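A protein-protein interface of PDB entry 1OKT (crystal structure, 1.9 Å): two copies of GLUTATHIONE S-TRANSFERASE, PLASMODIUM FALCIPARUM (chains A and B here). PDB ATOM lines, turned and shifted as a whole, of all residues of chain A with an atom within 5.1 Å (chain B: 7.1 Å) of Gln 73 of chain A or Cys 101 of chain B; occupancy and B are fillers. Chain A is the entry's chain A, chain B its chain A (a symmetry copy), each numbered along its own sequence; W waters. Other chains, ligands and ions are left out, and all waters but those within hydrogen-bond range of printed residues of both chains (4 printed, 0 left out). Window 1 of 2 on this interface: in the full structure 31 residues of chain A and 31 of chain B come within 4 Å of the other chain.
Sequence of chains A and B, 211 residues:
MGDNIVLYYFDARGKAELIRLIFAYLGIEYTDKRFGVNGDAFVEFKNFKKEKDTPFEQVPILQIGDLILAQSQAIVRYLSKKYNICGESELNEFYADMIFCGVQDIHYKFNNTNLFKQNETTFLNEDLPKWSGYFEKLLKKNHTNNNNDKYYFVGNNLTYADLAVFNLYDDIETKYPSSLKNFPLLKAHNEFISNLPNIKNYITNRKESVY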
ATOM      1  N   GLN A  71      -4.053   7.028 -31.239  1.00  0.00           N
ATOM      2  CA  GLN A  71      -3.049   8.078 -31.060  1.00  0.00           C
ATOM      3  C   GLN A  71      -1.810   7.768 -31.888  1.00  0.00           C
ATOM      4  O   GLN A  71      -0.983   6.944 -31.508  1.00  0.00           O
ATOM      5  CB  GLN A  71      -2.687   8.251 -29.581  1.00  0.00           C
ATOM      6  CG  GLN A  71      -3.770   8.943 -28.743  1.00  0.00           C
ATOM      7  CD  GLN A  71      -4.051  10.376 -29.182  1.00  0.00           C
ATOM      8  OE1 GLN A  71      -3.329  10.946 -29.999  1.00  0.00           O
ATOM      9  NE2 GLN A  71      -5.099  10.965 -28.627  1.00  0.00           N
ATOM     10  N   SER A  72      -1.710   8.424 -33.037  1.00  0.00           N
ATOM     11  CA  SER A  72      -0.595   8.208 -33.955  1.00  0.00           C
ATOM     12  C   SER A  72       0.789   8.153 -33.324  1.00  0.00           C
ATOM     13  O   SER A  72       1.567   7.256 -33.641  1.00  0.00           O
ATOM     14  CB  SER A  72      -0.610   9.272 -35.053  1.00  0.00           C
ATOM     15  OG  SER A  72      -0.473  10.575 -34.513  1.00  0.00           O
ATOM     16  N   GLN A  73       1.117   9.098 -32.444  1.00  0.00           N
ATOM     17  CA  GLN A  73       2.452   9.089 -31.841  1.00  0.00           C
ATOM     18  C   GLN A  73       2.698   7.849 -30.991  1.00  0.00           C
ATOM     19  O   GLN A  73       3.782   7.264 -31.028  1.00  0.00           O
ATOM     20  CB  GLN A  73       2.690  10.333 -30.977  1.00  0.00           C
ATOM     21  CG  GLN A  73       2.411  11.652 -31.658  1.00  0.00           C
ATOM     22  CD  GLN A  73       1.096  12.244 -31.204  1.00  0.00           C
ATOM     23  OE1 GLN A  73       1.050  13.345 -30.642  1.00  0.00           O
ATOM     24  NE2 GLN A  73       0.020  11.511 -31.421  1.00  0.00           N
ATOM     25  N   ALA A  74       1.700   7.462 -30.207  1.00  0.00           N
ATOM     26  CA  ALA A  74       1.841   6.303 -29.343  1.00  0.00           C
ATOM     27  C   ALA A  74       1.967   5.039 -30.181  1.00  0.00           C
ATOM     28  O   ALA A  74       2.720   4.125 -29.835  1.00  0.00           O
ATOM     29  CB  ALA A  74       0.651   6.206 -28.399  1.00  0.00           C
ATOM     30  N   ILE A  75       1.239   4.992 -31.291  1.00  0.00           N
ATOM     31  CA  ILE A  75       1.301   3.838 -32.183  1.00  0.00           C
ATOM     32  C   ILE A  75       2.701   3.711 -32.781  1.00  0.00           C
ATOM     33  O   ILE A  75       3.268   2.620 -32.839  1.00  0.00           O
ATOM     34  CB  ILE A  75       0.274   3.972 -33.317  1.00  0.00           C
ATOM     35  CG1 ILE A  75      -1.143   3.843 -32.732  1.00  0.00           C
ATOM     36  CG2 ILE A  75       0.538   2.915 -34.390  1.00  0.00           C
ATOM     37  CD1 ILE A  75      -2.248   4.203 -33.693  1.00  0.00           C
ATOM     38  N   VAL A  76       3.251   4.834 -33.230  1.00  0.00           N
ATOM     39  CA  VAL A  76       4.592   4.854 -33.816  1.00  0.00           C
ATOM     40  C   VAL A  76       5.636   4.346 -32.823  1.00  0.00           C
ATOM     41  O   VAL A  76       6.504   3.544 -33.176  1.00  0.00           O
ATOM     42  CB  VAL A  76       4.970   6.290 -34.274  1.00  0.00           C
ATOM     43  CG1 VAL A  76       6.479   6.398 -34.509  1.00  0.00           C
ATOM     44  CG2 VAL A  76       4.214   6.637 -35.548  1.00  0.00           C
ATOM     45  N   ARG A  77       5.560   4.812 -31.581  1.00  0.00           N
ATOM     46  CA  ARG A  77       6.508   4.366 -30.570  1.00  0.00           C
ATOM     47  C   ARG A  77       6.301   2.892 -30.206  1.00  0.00           C
ATOM     48  O   ARG A  77       7.257   2.188 -29.881  1.00  0.00           O
ATOM     49  CB  ARG A  77       6.405   5.242 -29.317  1.00  0.00           C
ATOM     50  CG  ARG A  77       7.067   6.612 -29.475  1.00  0.00           C
ATOM     51  CD  ARG A  77       7.015   7.408 -28.171  1.00  0.00           C
ATOM     52  NE  ARG A  77       5.686   7.944 -27.899  1.00  0.00           N
ATOM     53  CZ  ARG A  77       5.229   9.089 -28.398  1.00  0.00           C
ATOM     54  NH1 ARG A  77       5.998   9.816 -29.195  1.00  0.00           N
ATOM     55  NH2 ARG A  77       4.014   9.519 -28.081  1.00  0.00           N
ATOM     56  N   TYR A  78       5.056   2.428 -30.261  1.00  0.00           N
ATOM     57  CA  TYR A  78       4.753   1.031 -29.934  1.00  0.00           C
ATOM     58  C   TYR A  78       5.362   0.082 -30.962  1.00  0.00           C
ATOM     59  O   TYR A  78       5.999  -0.916 -30.615  1.00  0.00           O
ATOM     60  CB  TYR A  78       3.241   0.818 -29.890  1.00  0.00           C
ATOM     61  CG  TYR A  78       2.836  -0.634 -29.746  1.00  0.00           C
ATOM     62  CD1 TYR A  78       2.854  -1.267 -28.504  1.00  0.00           C
ATOM     63  CD2 TYR A  78       2.447  -1.376 -30.859  1.00  0.00           C
ATOM     64  CE1 TYR A  78       2.490  -2.613 -28.371  1.00  0.00           C
ATOM     65  CE2 TYR A  78       2.083  -2.719 -30.742  1.00  0.00           C
ATOM     66  CZ  TYR A  78       2.108  -3.330 -29.494  1.00  0.00           C
ATOM     67  OH  TYR A  78       1.761  -4.658 -29.380  1.00  0.00           O
ATOM     68  N   PHE A 100      11.501  13.140 -32.871  1.00  0.00           N
ATOM     69  CA  PHE A 100      10.127  12.977 -33.351  1.00  0.00           C
ATOM     70  C   PHE A 100       9.259  14.104 -32.788  1.00  0.00           C
ATOM     71  O   PHE A 100       8.398  14.635 -33.484  1.00  0.00           O
ATOM     72  CB  PHE A 100       9.569  11.605 -32.939  1.00  0.00           C
ATOM     73  CG  PHE A 100       8.164  11.337 -33.420  1.00  0.00           C
ATOM     74  CD1 PHE A 100       7.747  11.745 -34.684  1.00  0.00           C
ATOM     75  CD2 PHE A 100       7.263  10.639 -32.610  1.00  0.00           C
ATOM     76  CE1 PHE A 100       6.457  11.469 -35.143  1.00  0.00           C
ATOM     77  CE2 PHE A 100       5.969  10.355 -33.057  1.00  0.00           C
ATOM     78  CZ  PHE A 100       5.565  10.771 -34.327  1.00  0.00           C
ATOM     79  N   GLN A 104       7.000  16.845 -35.036  1.00  0.00           N
ATOM     80  CA  GLN A 104       5.577  17.124 -34.852  1.00  0.00           C
ATOM     81  C   GLN A 104       5.313  18.627 -34.828  1.00  0.00           C
ATOM     82  O   GLN A 104       4.328  19.109 -35.396  1.00  0.00           O
ATOM     83  CB  GLN A 104       5.076  16.486 -33.545  1.00  0.00           C
ATOM     84  CG  GLN A 104       5.108  14.961 -33.545  1.00  0.00           C
ATOM     85  CD  GLN A 104       4.760  14.357 -32.194  1.00  0.00           C
ATOM     86  OE1 GLN A 104       5.505  13.529 -31.662  1.00  0.00           O
ATOM     87  NE2 GLN A 104       3.624  14.761 -31.635  1.00  0.00           N
ATOM     88  N   GLN B  73       7.624  16.290 -23.936  1.00  0.00           N
ATOM     89  CA  GLN B  73       7.066  14.936 -23.981  1.00  0.00           C
ATOM     90  C   GLN B  73       8.140  13.861 -23.885  1.00  0.00           C
ATOM     91  O   GLN B  73       7.965  12.854 -23.196  1.00  0.00           O
ATOM     92  CB  GLN B  73       6.251  14.703 -25.259  1.00  0.00           C
ATOM     93  CG  GLN B  73       5.188  15.739 -25.541  1.00  0.00           C
ATOM     94  CD  GLN B  73       5.619  16.696 -26.629  1.00  0.00           C
ATOM     95  OE1 GLN B  73       4.979  16.797 -27.683  1.00  0.00           O
ATOM     96  NE2 GLN B  73       6.718  17.387 -26.395  1.00  0.00           N
ATOM     97  N   ARG B  77       8.663  10.965 -20.867  1.00  0.00           N
ATOM     98  CA  ARG B  77       8.785   9.534 -21.110  1.00  0.00           C
ATOM     99  C   ARG B  77      10.142   8.993 -20.650  1.00  0.00           C
ATOM    100  O   ARG B  77      10.243   7.844 -20.217  1.00  0.00           O
ATOM    101  CB  ARG B  77       8.566   9.224 -22.595  1.00  0.00           C
ATOM    102  CG  ARG B  77       7.096   9.270 -23.017  1.00  0.00           C
ATOM    103  CD  ARG B  77       6.925   8.866 -24.481  1.00  0.00           C
ATOM    104  NE  ARG B  77       7.350   9.915 -25.401  1.00  0.00           N
ATOM    105  CZ  ARG B  77       6.576  10.926 -25.785  1.00  0.00           C
ATOM    106  NH1 ARG B  77       5.337  11.023 -25.325  1.00  0.00           N
ATOM    107  NH2 ARG B  77       7.032  11.828 -26.645  1.00  0.00           N
ATOM    108  N   PHE B  94       2.196   1.318 -23.747  1.00  0.00           N
ATOM    109  CA  PHE B  94       1.465   1.942 -24.840  1.00  0.00           C
ATOM    110  C   PHE B  94       0.240   2.705 -24.319  1.00  0.00           C
ATOM    111  O   PHE B  94       0.005   3.850 -24.699  1.00  0.00           O
ATOM    112  CB  PHE B  94       0.990   0.903 -25.854  1.00  0.00           C
ATOM    113  CG  PHE B  94      -0.088   1.419 -26.755  1.00  0.00           C
ATOM    114  CD1 PHE B  94       0.226   2.243 -27.832  1.00  0.00           C
ATOM    115  CD2 PHE B  94      -1.424   1.187 -26.454  1.00  0.00           C
ATOM    116  CE1 PHE B  94      -0.778   2.837 -28.594  1.00  0.00           C
ATOM    117  CE2 PHE B  94      -2.436   1.779 -27.211  1.00  0.00           C
ATOM    118  CZ  PHE B  94      -2.110   2.606 -28.281  1.00  0.00           C
ATOM    119  N   TYR B  95      -0.552   2.070 -23.460  1.00  0.00           N
ATOM    120  CA  TYR B  95      -1.744   2.737 -22.937  1.00  0.00           C
ATOM    121  C   TYR B  95      -1.416   4.034 -22.204  1.00  0.00           C
ATOM    122  O   TYR B  95      -2.102   5.041 -22.390  1.00  0.00           O
ATOM    123  CB  TYR B  95      -2.547   1.784 -22.037  1.00  0.00           C
ATOM    124  CG  TYR B  95      -3.298   0.712 -22.809  1.00  0.00           C
ATOM    125  CD1 TYR B  95      -3.365  -0.605 -22.340  1.00  0.00           C
ATOM    126  CD2 TYR B  95      -3.937   1.012 -24.012  1.00  0.00           C
ATOM    127  CE1 TYR B  95      -4.046  -1.595 -23.054  1.00  0.00           C
ATOM    128  CE2 TYR B  95      -4.621   0.027 -24.738  1.00  0.00           C
ATOM    129  CZ  TYR B  95      -4.668  -1.271 -24.252  1.00  0.00           C
ATOM    130  OH  TYR B  95      -5.321  -2.243 -24.976  1.00  0.00           O
ATOM    131  N   ALA B  96      -0.366   4.036 -21.387  1.00  0.00           N
ATOM    132  CA  ALA B  96       0.006   5.261 -20.672  1.00  0.00           C
ATOM    133  C   ALA B  96       0.367   6.342 -21.699  1.00  0.00           C
ATOM    134  O   ALA B  96       0.035   7.518 -21.536  1.00  0.00           O
ATOM    135  CB  ALA B  96       1.191   5.000 -19.745  1.00  0.00           C
ATOM    136  N   ASP B  97       1.042   5.911 -22.758  1.00  0.00           N
ATOM    137  CA  ASP B  97       1.470   6.781 -23.851  1.00  0.00           C
ATOM    138  C   ASP B  97       0.251   7.363 -24.583  1.00  0.00           C
ATOM    139  O   ASP B  97       0.148   8.574 -24.801  1.00  0.00           O
ATOM    140  CB  ASP B  97       2.307   5.954 -24.832  1.00  0.00           C
ATOM    141  CG  ASP B  97       3.088   6.803 -25.812  1.00  0.00           C
ATOM    142  OD1 ASP B  97       2.767   7.998 -25.985  1.00  0.00           O
ATOM    143  OD2 ASP B  97       4.024   6.257 -26.424  1.00  0.00           O
ATOM    144  N   MET B  98      -0.660   6.481 -24.973  1.00  0.00           N
ATOM    145  CA  MET B  98      -1.873   6.873 -25.684  1.00  0.00           C
ATOM    146  C   MET B  98      -2.652   7.918 -24.878  1.00  0.00           C
ATOM    147  O   MET B  98      -3.123   8.923 -25.416  1.00  0.00           O
ATOM    148  CB  MET B  98      -2.722   5.618 -25.938  1.00  0.00           C
ATOM    149  CG  MET B  98      -4.020   5.883 -26.666  1.00  0.00           C
ATOM    150  SD  MET B  98      -5.056   4.429 -26.645  1.00  0.00           S
ATOM    151  CE  MET B  98      -5.758   4.557 -25.004  1.00  0.00           C
ATOM    152  N   ILE B  99      -2.767   7.688 -23.578  1.00  0.00           N
ATOM    153  CA  ILE B  99      -3.483   8.613 -22.718  1.00  0.00           C
ATOM    154  C   ILE B  99      -2.783   9.968 -22.670  1.00  0.00           C
ATOM    155  O   ILE B  99      -3.440  11.005 -22.734  1.00  0.00           O
ATOM    156  CB  ILE B  99      -3.645   8.014 -21.303  1.00  0.00           C
ATOM    157  CG1 ILE B  99      -4.591   6.808 -21.393  1.00  0.00           C
ATOM    158  CG2 ILE B  99      -4.166   9.072 -20.331  1.00  0.00           C
ATOM    159  CD1 ILE B  99      -4.666   5.937 -20.147  1.00  0.00           C
ATOM    160  N   PHE B 100      -1.456   9.962 -22.573  1.00  0.00           N
ATOM    161  CA  PHE B 100      -0.706  11.220 -22.542  1.00  0.00           C
ATOM    162  C   PHE B 100      -0.902  11.957 -23.868  1.00  0.00           C
ATOM    163  O   PHE B 100      -1.040  13.177 -23.888  1.00  0.00           O
ATOM    164  CB  PHE B 100       0.786  10.953 -22.283  1.00  0.00           C
ATOM    165  CG  PHE B 100       1.632  12.200 -22.203  1.00  0.00           C
ATOM    166  CD1 PHE B 100       1.160  13.350 -21.576  1.00  0.00           C
ATOM    167  CD2 PHE B 100       2.928  12.207 -22.731  1.00  0.00           C
ATOM    168  CE1 PHE B 100       1.956  14.494 -21.472  1.00  0.00           C
ATOM    169  CE2 PHE B 100       3.734  13.345 -22.633  1.00  0.00           C
ATOM    170  CZ  PHE B 100       3.248  14.491 -22.002  1.00  0.00           C
ATOM    171  N   CYS B 101      -0.909  11.224 -24.979  1.00  0.00           N
ATOM    172  CA  CYS B 101      -1.134  11.868 -26.271  1.00  0.00           C
ATOM    173  C   CYS B 101      -2.517  12.527 -26.282  1.00  0.00           C
ATOM    174  O   CYS B 101      -2.691  13.626 -26.819  1.00  0.00           O
ATOM    175  CB  CYS B 101      -1.030  10.860 -27.411  1.00  0.00           C
ATOM    176  SG  CYS B 101       0.675  10.291 -27.693  1.00  0.00           S
ATOM    177  N   GLY B 102      -3.503  11.853 -25.699  1.00  0.00           N
ATOM    178  CA  GLY B 102      -4.840  12.436 -25.639  1.00  0.00           C
ATOM    179  C   GLY B 102      -4.836  13.725 -24.824  1.00  0.00           C
ATOM    180  O   GLY B 102      -5.432  14.736 -25.214  1.00  0.00           O
ATOM    181  N   VAL B 103      -4.165  13.693 -23.679  1.00  0.00           N
ATOM    182  CA  VAL B 103      -4.069  14.862 -22.808  1.00  0.00           C
ATOM    183  C   VAL B 103      -3.481  16.076 -23.558  1.00  0.00           C
ATOM    184  O   VAL B 103      -3.977  17.197 -23.433  1.00  0.00           O
ATOM    185  CB  VAL B 103      -3.178  14.551 -21.561  1.00  0.00           C
ATOM    186  CG1 VAL B 103      -2.923  15.821 -20.750  1.00  0.00           C
ATOM    187  CG2 VAL B 103      -3.879  13.514 -20.657  1.00  0.00           C
ATOM    188  N   GLN B 104      -2.425  15.848 -24.332  1.00  0.00           N
ATOM    189  CA  GLN B 104      -1.779  16.929 -25.073  1.00  0.00           C
ATOM    190  C   GLN B 104      -2.771  17.628 -25.997  1.00  0.00           C
ATOM    191  O   GLN B 104      -2.762  18.856 -26.129  1.00  0.00           O
ATOM    192  CB  GLN B 104      -0.600  16.378 -25.894  1.00  0.00           C
ATOM    193  CG  GLN B 104       0.548  15.836 -25.047  1.00  0.00           C
ATOM    194  CD  GLN B 104       1.628  15.156 -25.874  1.00  0.00           C
ATOM    195  OE1 GLN B 104       2.006  14.013 -25.600  1.00  0.00           O
ATOM    196  NE2 GLN B 104       2.135  15.855 -26.884  1.00  0.00           N
ATOM    197  N   ASP B 105      -3.625  16.839 -26.634  1.00  0.00           N
ATOM    198  CA  ASP B 105      -4.637  17.365 -27.544  1.00  0.00           C
ATOM    199  C   ASP B 105      -5.560  18.343 -26.827  1.00  0.00           C
ATOM    200  O   ASP B 105      -5.682  19.492 -27.228  1.00  0.00           O
ATOM    201  CB  ASP B 105      -5.464  16.216 -28.127  1.00  0.00           C
ATOM    202  CG  ASP B 105      -6.423  16.667 -29.221  1.00  0.00           C
ATOM    203  OD1 ASP B 105      -7.145  17.661 -29.018  1.00  0.00           O
ATOM    204  OD2 ASP B 105      -6.466  16.015 -30.283  1.00  0.00           O
ATOM    205  N   ILE B 106      -6.185  17.902 -25.743  1.00  0.00           N
ATOM    206  CA  ILE B 106      -7.112  18.776 -25.041  1.00  0.00           C
ATOM    207  C   ILE B 106      -6.417  19.881 -24.246  1.00  0.00           C
ATOM    208  O   ILE B 106      -6.960  20.980 -24.110  1.00  0.00           O
ATOM    209  CB  ILE B 106      -8.091  17.936 -24.155  1.00  0.00           C
ATOM    210  CG1 ILE B 106      -9.172  18.840 -23.561  1.00  0.00           C
ATOM    211  CG2 ILE B 106      -7.318  17.162 -23.097  1.00  0.00           C
ATOM    212  CD1 ILE B 106     -10.055  19.507 -24.600  1.00  0.00           C
ATOM    213  N   TRP B 131     -13.981  15.374 -24.062  1.00  0.00           N
ATOM    214  CA  TRP B 131     -12.737  14.764 -23.602  1.00  0.00           C
ATOM    215  C   TRP B 131     -12.807  14.241 -22.167  1.00  0.00           C
ATOM    216  O   TRP B 131     -12.186  13.233 -21.842  1.00  0.00           O
ATOM    217  CB  TRP B 131     -11.572  15.742 -23.773  1.00  0.00           C
ATOM    218  CG  TRP B 131     -11.139  15.821 -25.209  1.00  0.00           C
ATOM    219  CD1 TRP B 131     -11.699  16.578 -26.200  1.00  0.00           C
ATOM    220  CD2 TRP B 131     -10.115  15.040 -25.833  1.00  0.00           C
ATOM    221  NE1 TRP B 131     -11.090  16.313 -27.406  1.00  0.00           N
ATOM    222  CE2 TRP B 131     -10.113  15.373 -27.209  1.00  0.00           C
ATOM    223  CE3 TRP B 131      -9.200  14.086 -25.363  1.00  0.00           C
ATOM    224  CZ2 TRP B 131      -9.226  14.788 -28.123  1.00  0.00           C
ATOM    225  CZ3 TRP B 131      -8.316  13.500 -26.275  1.00  0.00           C
ATOM    226  CH2 TRP B 131      -8.340  13.857 -27.639  1.00  0.00           C
ATOM    227  N   PHE B 135     -11.859  10.339 -20.946  1.00  0.00           N
ATOM    228  CA  PHE B 135     -11.043   9.958 -19.805  1.00  0.00           C
ATOM    229  C   PHE B 135     -11.840   9.177 -18.766  1.00  0.00           C
ATOM    230  O   PHE B 135     -11.329   8.218 -18.184  1.00  0.00           O
ATOM    231  CB  PHE B 135     -10.413  11.205 -19.178  1.00  0.00           C
ATOM    232  CG  PHE B 135      -9.406  11.887 -20.075  1.00  0.00           C
ATOM    233  CD1 PHE B 135      -9.498  13.250 -20.344  1.00  0.00           C
ATOM    234  CD2 PHE B 135      -8.355  11.164 -20.636  1.00  0.00           C
ATOM    235  CE1 PHE B 135      -8.553  13.882 -21.156  1.00  0.00           C
ATOM    236  CE2 PHE B 135      -7.408  11.788 -21.448  1.00  0.00           C
ATOM    237  CZ  PHE B 135      -7.509  13.149 -21.707  1.00  0.00           C
ATOM    238  N   TYR B 160       2.890   8.064 -15.444  1.00  0.00           N
ATOM    239  CA  TYR B 160       2.930   9.489 -15.732  1.00  0.00           C
ATOM    240  C   TYR B 160       1.589   9.915 -16.314  1.00  0.00           C
ATOM    241  O   TYR B 160       1.214  11.083 -16.244  1.00  0.00           O
ATOM    242  CB  TYR B 160       4.083   9.812 -16.698  1.00  0.00           C
ATOM    243  CG  TYR B 160       3.990   9.166 -18.066  1.00  0.00           C
ATOM    244  CD1 TYR B 160       3.462   9.863 -19.154  1.00  0.00           C
ATOM    245  CD2 TYR B 160       4.448   7.869 -18.274  1.00  0.00           C
ATOM    246  CE1 TYR B 160       3.394   9.277 -20.422  1.00  0.00           C
ATOM    247  CE2 TYR B 160       4.382   7.272 -19.534  1.00  0.00           C
ATOM    248  CZ  TYR B 160       3.857   7.981 -20.601  1.00  0.00           C
ATOM    249  OH  TYR B 160       3.831   7.402 -21.848  1.00  0.00           O
HETATM  250  O   HOH W   1      -6.142  13.184 -29.377  1.00  0.00           O
HETATM  251  O   HOH W   2      -1.555  14.065 -29.399  1.00  0.00           O
HETATM  252  O   HOH W   3      -4.562  13.486 -31.422  1.00  0.00           O
HETATM  253  O   HOH W   4       3.469   3.725 -27.334  1.00  0.00           O
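NH1 of Arg 77 of chain B lies close to NH2 of Arg 77 of chain A, at 3.4 Å.
The side-chain sulfur (SG) of Cys 101 of chain B is in hydrogen-bond range of the guanidinium group (NH2) of Arg 77 of chain A.
NE of Arg 77 of chain A lies within salt-bridge range of OD2 of Asp 97 of chain B, 2.8 Å away.
NE2 of Gln 71 of chain A lies close to N of Gly 102 of chain B, at 3.5 Å.
NE2 of Gln 104 of chain A lies within hydrogen-bond range of OE1 of Gln 73 of chain A.
The side-chain hydroxyl (OG) of Ser 72 of chain A is in hydrogen-bond range of the side-chain amide nitrogen (NE2) of Gln 73 of chain A (3.3 Å).
The backbone NH of Asp 97 of chain B lies close to the side-chain hydroxyl of Tyr 160 of chain B (3.3 Å).
The backbone carbonyl oxygen of Asp 97 of chain B sits at hydrogen-bond distance from the side-chain sulfur of Cys 101 of chain B, at 3.4 Å.
Among the printed residues, pairs that only touch across the chains: Gln 71 of chain A with Met 98 of chain B (3.4 Å), Gln 71 of chain A with Cys 101 of chain B (3.5 Å), Ala 74 of chain A with Asp 97 of chain B (3.6 Å), Ala 74 of chain A with Phe 94 of chain B (3.7 Å), Ala 74 of chain A with Met 98 of chain B (3.7 Å), Gln 73 of chain A with Cys 101 of chain B (3.9 Å), Tyr 78 of chain A with Phe 94 of chain B (3.9 Å), Ala 74 of chain A with Cys 101 of chain B (3.9 Å) and Ile 75 of chain A with Phe 94 of chain B (3.998 Å).
Gln 73 of chain A touches one residue of chain B.
Of chain A, only Gln 71, Gln 73, Ala 74 and Arg 77 come within 4 Å of Cys 101 of chain B.
Printed residues of chain B within 4 Å of Arg 77 of chain A: Arg 77, Asp 97 and Cys 101.
Of the printed residues of chain B, Ala 74 of chain A touches Phe 94 (3.7 Å), Asp 97 (3.6 Å), Met 98 (3.7 Å) and Cys 101 (3.9 Å).
Of the printed residues of chain A, Phe 94 of chain B touches Ala 74, Ile 75 and Tyr 78.
Of the printed residues of chain B, Ile 75 of chain A touches Phe 94 (3.998 Å).
Of the printed residues of chain B, Gln 71 of chain A touches Met 98 (3.4 Å), Cys 101 (3.5 Å) and Gly 102 (3.3 Å).
Phe 100 of chain B touches none of the printed residues of chain A.
The nearest residue of chain B that does not touch Gln 73 of chain A is Gln 104 of chain B (4.6 Å).
The nearest printed residue of chain A that does not touch Cys 101 of chain B is Ser 72 of chain A (6.0 Å).
Printed residues of chain A that touch a printed residue of chain B: Gln 71, Gln 73, Ala 74, Ile 75, Arg 77 and Tyr 78.
Of the 18 printed residues of chain B, 6 touch a printed residue of chain A.
Along chain B the printed residues that touch a printed residue of chain A span positions 77 to 102.
Among the printed residues, 13 pairs touch across the chains.
Among the printed residues, Asp or Glu carboxylates within 4 Å of a Lys or Arg side-chain nitrogen of the other chain: Arg 77 of chain A with Asp 97 of chain B.
Arg 77 of chain A touches its own counterpart, Arg 77 of chain B.
Positions printed for both chains: 73, 77, 100 and 104.
Water W1 lies within hydrogen-bond range of NE2 of Gln 71 of chain A and OD2 of Asp 105 of chain B.
Water W4 lies within hydrogen-bond range of the backbone carbonyl oxygen (O) of Ala 74 of chain A (2.6 Å) and the side-chain carboxylate (OD2) of Asp 97 of chain B (2.7 Å).
Water W2 bridges O of Cys 101 of chain B (2.9 Å) and OE1 of Gln 73 of chain A (3.0 Å).
Water W3 lies within hydrogen-bond range of the side-chain amide oxygen (OE1) of Gln 71 of chain A (3.2 Å) and the side-chain carboxylate (OD2) of Asp 105 of chain B (3.4 Å).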
